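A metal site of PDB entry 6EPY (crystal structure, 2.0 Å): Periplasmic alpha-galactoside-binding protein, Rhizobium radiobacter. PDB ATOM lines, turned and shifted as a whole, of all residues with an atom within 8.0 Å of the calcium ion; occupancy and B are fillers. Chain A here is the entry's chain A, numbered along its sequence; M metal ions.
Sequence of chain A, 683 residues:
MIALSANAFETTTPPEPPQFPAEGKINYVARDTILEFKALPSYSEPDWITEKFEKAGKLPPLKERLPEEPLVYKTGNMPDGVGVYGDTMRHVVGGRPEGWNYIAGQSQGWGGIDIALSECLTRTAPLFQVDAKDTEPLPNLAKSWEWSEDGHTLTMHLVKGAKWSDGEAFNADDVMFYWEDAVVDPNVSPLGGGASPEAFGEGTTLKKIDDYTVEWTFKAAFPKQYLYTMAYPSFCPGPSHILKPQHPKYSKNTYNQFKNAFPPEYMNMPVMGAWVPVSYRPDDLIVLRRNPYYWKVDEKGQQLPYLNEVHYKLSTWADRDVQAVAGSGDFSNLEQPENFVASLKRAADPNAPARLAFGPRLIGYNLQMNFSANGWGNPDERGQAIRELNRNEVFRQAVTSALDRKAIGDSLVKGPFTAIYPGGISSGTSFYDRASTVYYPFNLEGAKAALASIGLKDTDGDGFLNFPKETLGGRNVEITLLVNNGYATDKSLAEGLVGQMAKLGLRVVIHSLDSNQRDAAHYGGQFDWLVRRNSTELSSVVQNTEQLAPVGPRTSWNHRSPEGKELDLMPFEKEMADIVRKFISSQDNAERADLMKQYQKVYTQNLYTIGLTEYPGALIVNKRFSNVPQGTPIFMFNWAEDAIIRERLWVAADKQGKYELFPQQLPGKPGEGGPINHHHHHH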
ATOM      1  N   LYS A 457      18.351  13.520 -13.391  1.00  0.00           N
ATOM      2  CA  LYS A 457      18.849  12.437 -12.550  1.00  0.00           C
ATOM      3  C   LYS A 457      19.447  12.985 -11.231  1.00  0.00           C
ATOM      4  O   LYS A 457      19.997  14.080 -11.223  1.00  0.00           O
ATOM      5  CB  LYS A 457      19.883  11.613 -13.376  1.00  0.00           C
ATOM      6  CG  LYS A 457      20.650  10.540 -12.649  1.00  0.00           C
ATOM      7  CD  LYS A 457      21.808  10.135 -13.512  1.00  0.00           C
ATOM      8  CE  LYS A 457      22.869   9.440 -12.725  1.00  0.00           C
ATOM      9  NZ  LYS A 457      24.218   9.835 -13.207  1.00  0.00           N
ATOM     10  N   ASP A 458      19.333  12.207 -10.134  1.00  0.00           N
ATOM     11  CA  ASP A 458      19.869  12.571  -8.828  1.00  0.00           C
ATOM     12  C   ASP A 458      21.368  12.319  -8.837  1.00  0.00           C
ATOM     13  O   ASP A 458      21.794  11.167  -8.906  1.00  0.00           O
ATOM     14  CB  ASP A 458      19.147  11.787  -7.707  1.00  0.00           C
ATOM     15  CG  ASP A 458      19.618  12.053  -6.287  1.00  0.00           C
ATOM     16  OD1 ASP A 458      20.095  13.176  -6.012  1.00  0.00           O
ATOM     17  OD2 ASP A 458      19.442  11.166  -5.429  1.00  0.00           O
ATOM     18  N   THR A 459      22.156  13.400  -8.871  1.00  0.00           N
ATOM     19  CA  THR A 459      23.621  13.345  -8.950  1.00  0.00           C
ATOM     20  C   THR A 459      24.305  13.585  -7.588  1.00  0.00           C
ATOM     21  O   THR A 459      25.529  13.580  -7.529  1.00  0.00           O
ATOM     22  CB  THR A 459      24.152  14.284 -10.064  1.00  0.00           C
ATOM     23  OG1 THR A 459      23.730  15.625  -9.799  1.00  0.00           O
ATOM     24  CG2 THR A 459      23.701  13.858 -11.468  1.00  0.00           C
ATOM     25  N   ASP A 460      23.526  13.798  -6.501  1.00  0.00           N
ATOM     26  CA  ASP A 460      24.113  14.062  -5.178  1.00  0.00           C
ATOM     27  C   ASP A 460      23.558  13.119  -4.061  1.00  0.00           C
ATOM     28  O   ASP A 460      23.797  13.355  -2.871  1.00  0.00           O
ATOM     29  CB  ASP A 460      24.007  15.560  -4.816  1.00  0.00           C
ATOM     30  CG  ASP A 460      22.667  16.221  -5.050  1.00  0.00           C
ATOM     31  OD1 ASP A 460      21.648  15.596  -4.732  1.00  0.00           O
ATOM     32  OD2 ASP A 460      22.634  17.400  -5.475  1.00  0.00           O
ATOM     33  N   GLY A 461      22.836  12.078  -4.467  1.00  0.00           N
ATOM     34  CA  GLY A 461      22.242  11.074  -3.592  1.00  0.00           C
ATOM     35  C   GLY A 461      21.196  11.519  -2.579  1.00  0.00           C
ATOM     36  O   GLY A 461      20.911  10.786  -1.617  1.00  0.00           O
ATOM     37  N   ASP A 462      20.584  12.722  -2.757  1.00  0.00           N
ATOM     38  CA  ASP A 462      19.593  13.196  -1.793  1.00  0.00           C
ATOM     39  C   ASP A 462      18.143  12.787  -2.152  1.00  0.00           C
ATOM     40  O   ASP A 462      17.198  13.226  -1.486  1.00  0.00           O
ATOM     41  CB  ASP A 462      19.720  14.712  -1.528  1.00  0.00           C
ATOM     42  CG  ASP A 462      19.304  15.654  -2.650  1.00  0.00           C
ATOM     43  OD1 ASP A 462      19.002  15.170  -3.772  1.00  0.00           O
ATOM     44  OD2 ASP A 462      19.297  16.882  -2.420  1.00  0.00           O
ATOM     45  N   GLY A 463      17.986  11.956  -3.181  1.00  0.00           N
ATOM     46  CA  GLY A 463      16.678  11.486  -3.644  1.00  0.00           C
ATOM     47  C   GLY A 463      15.901  12.464  -4.522  1.00  0.00           C
ATOM     48  O   GLY A 463      14.821  12.120  -4.985  1.00  0.00           O
ATOM     49  N   PHE A 464      16.454  13.666  -4.741  1.00  0.00           N
ATOM     50  CA  PHE A 464      15.856  14.689  -5.578  1.00  0.00           C
ATOM     51  C   PHE A 464      16.617  14.838  -6.880  1.00  0.00           C
ATOM     52  O   PHE A 464      17.841  14.859  -6.887  1.00  0.00           O
ATOM     53  CB  PHE A 464      15.717  16.031  -4.851  1.00  0.00           C
ATOM     54  CG  PHE A 464      14.663  16.011  -3.776  1.00  0.00           C
ATOM     55  CD1 PHE A 464      13.314  16.046  -4.109  1.00  0.00           C
ATOM     56  CD2 PHE A 464      15.006  15.941  -2.437  1.00  0.00           C
ATOM     57  CE1 PHE A 464      12.336  16.023  -3.110  1.00  0.00           C
ATOM     58  CE2 PHE A 464      14.027  15.924  -1.450  1.00  0.00           C
ATOM     59  CZ  PHE A 464      12.699  15.984  -1.791  1.00  0.00           C
ATOM     60  N   LEU A 465      15.888  14.902  -7.984  1.00  0.00           N
ATOM     61  CA  LEU A 465      16.475  15.033  -9.316  1.00  0.00           C
ATOM     62  C   LEU A 465      17.183  16.368  -9.519  1.00  0.00           C
ATOM     63  O   LEU A 465      16.730  17.430  -9.063  1.00  0.00           O
ATOM     64  CB  LEU A 465      15.421  14.773 -10.411  1.00  0.00           C
ATOM     65  CG  LEU A 465      14.717  13.396 -10.361  1.00  0.00           C
ATOM     66  CD1 LEU A 465      13.616  13.329 -11.399  1.00  0.00           C
ATOM     67  CD2 LEU A 465      15.688  12.246 -10.549  1.00  0.00           C
ATOM     68  N   ASN A 466      18.333  16.287 -10.176  1.00  0.00           N
ATOM     69  CA  ASN A 466      19.164  17.425 -10.512  1.00  0.00           C
ATOM     70  C   ASN A 466      18.993  17.749 -11.980  1.00  0.00           C
ATOM     71  O   ASN A 466      18.776  16.839 -12.785  1.00  0.00           O
ATOM     72  CB  ASN A 466      20.632  17.095 -10.254  1.00  0.00           C
ATOM     73  CG  ASN A 466      20.997  17.005  -8.801  1.00  0.00           C
ATOM     74  OD1 ASN A 466      21.602  17.921  -8.256  1.00  0.00           O
ATOM     75  ND2 ASN A 466      20.602  15.936  -8.121  1.00  0.00           N
ATOM     76  N   PHE A 467      19.156  19.029 -12.332  1.00  0.00           N
ATOM     77  CA  PHE A 467      19.190  19.451 -13.730  1.00  0.00           C
ATOM     78  C   PHE A 467      20.496  18.893 -14.316  1.00  0.00           C
ATOM     79  O   PHE A 467      21.435  18.678 -13.549  1.00  0.00           O
ATOM     80  CB  PHE A 467      19.306  20.996 -13.812  1.00  0.00           C
ATOM     81  CG  PHE A 467      18.040  21.767 -13.589  1.00  0.00           C
ATOM     82  CD1 PHE A 467      17.049  21.802 -14.566  1.00  0.00           C
ATOM     83  CD2 PHE A 467      17.844  22.505 -12.433  1.00  0.00           C
ATOM     84  CE1 PHE A 467      15.876  22.542 -14.371  1.00  0.00           C
ATOM     85  CE2 PHE A 467      16.678  23.226 -12.225  1.00  0.00           C
ATOM     86  CZ  PHE A 467      15.707  23.261 -13.212  1.00  0.00           C
ATOM     87  N   GLY A 474      23.861  22.226 -12.576  1.00  0.00           N
ATOM     88  CA  GLY A 474      23.437  20.875 -12.226  1.00  0.00           C
ATOM     89  C   GLY A 474      22.819  20.735 -10.839  1.00  0.00           C
ATOM     90  O   GLY A 474      22.848  19.629 -10.270  1.00  0.00           O
ATOM     91  N   ARG A 475      22.243  21.828 -10.280  1.00  0.00           N
ATOM     92  CA  ARG A 475      21.596  21.817  -8.954  1.00  0.00           C
ATOM     93  C   ARG A 475      20.263  21.052  -9.000  1.00  0.00           C
ATOM     94  O   ARG A 475      19.741  20.752 -10.075  1.00  0.00           O
ATOM     95  CB  ARG A 475      21.383  23.264  -8.435  1.00  0.00           C
ATOM     96  CG  ARG A 475      20.208  23.981  -9.084  1.00  0.00           C
ATOM     97  CD  ARG A 475      19.999  25.392  -8.567  1.00  0.00           C
ATOM     98  NE  ARG A 475      21.017  26.276  -9.134  1.00  0.00           N
ATOM     99  CZ  ARG A 475      20.861  27.577  -9.296  1.00  0.00           C
ATOM    100  NH1 ARG A 475      19.746  28.179  -8.923  1.00  0.00           N
ATOM    101  NH2 ARG A 475      21.836  28.288  -9.843  1.00  0.00           N
ATOM    102  N   ASN A 476      19.688  20.774  -7.817  1.00  0.00           N
ATOM    103  CA  ASN A 476      18.372  20.121  -7.718  1.00  0.00           C
ATOM    104  C   ASN A 476      17.292  20.965  -8.378  1.00  0.00           C
ATOM    105  O   ASN A 476      17.285  22.193  -8.242  1.00  0.00           O
ATOM    106  CB  ASN A 476      17.991  19.922  -6.252  1.00  0.00           C
ATOM    107  CG  ASN A 476      18.590  18.713  -5.603  1.00  0.00           C
ATOM    108  OD1 ASN A 476      18.935  17.719  -6.247  1.00  0.00           O
ATOM    109  ND2 ASN A 476      18.651  18.739  -4.295  1.00  0.00           N
ATOM    110  N   VAL A 477      16.362  20.296  -9.076  1.00  0.00           N
ATOM    111  CA  VAL A 477      15.193  20.951  -9.660  1.00  0.00           C
ATOM    112  C   VAL A 477      14.335  21.418  -8.460  1.00  0.00           C
ATOM    113  O   VAL A 477      14.120  20.645  -7.512  1.00  0.00           O
ATOM    114  CB  VAL A 477      14.401  19.982 -10.595  1.00  0.00           C
ATOM    115  CG1 VAL A 477      13.116  20.614 -11.110  1.00  0.00           C
ATOM    116  CG2 VAL A 477      15.277  19.495 -11.752  1.00  0.00           C
ATOM    117  N   GLY A 505      10.784  12.286  -7.286  1.00  0.00           N
ATOM    118  CA  GLY A 505      12.091  12.919  -7.196  1.00  0.00           C
ATOM    119  C   GLY A 505      12.111  14.412  -7.492  1.00  0.00           C
ATOM    120  O   GLY A 505      13.170  15.008  -7.633  1.00  0.00           O
HETATM  121 CA    CA M   1      19.687  15.543  -5.911  1.00  0.00          CA
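The calcium ion is bound by the backbone carbonyl oxygen (O) of Phe 464 (2.2 Å), the side-chain carboxylate (OD1) of Asp 462 (2.3 Å), the side-chain carboxylate (OD1) of Asp 460 (2.3 Å), the side-chain amide oxygen (OD1) of Asn 476 (2.3 Å), the side-chain carboxylate (OD1) of Asp 458 (2.4 Å) and the side-chain amide nitrogen (ND2) of Asn 466 (2.4 Å).
Six residues have an atom within 4 Å of the calcium ion: Asp 458, Asp 460, Asp 462, Phe 464, Asn 466 and Asn 476.
The side-chain amide oxygen (OD1) of Asn 466 sits close to the backbone carbonyl oxygen (O) of Gly 474, at 2.9 Å.
The side-chain carboxylate (OD1) of Asp 458 lies close to the backbone NH (N) of Gly 461, at 3.3 Å.
The backbone carbonyl oxygen (O) of Lys 457 is in hydrogen-bond range of the backbone NH (N) of Asn 466.
OD2 of Asp 458 is in hydrogen-bond range of N of Gly 463, at 2.8 Å.
The side-chain hydroxyl (OG1) of Thr 459 sits close to the side-chain amide oxygen (OD1) of Asn 466 (3.5 Å).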
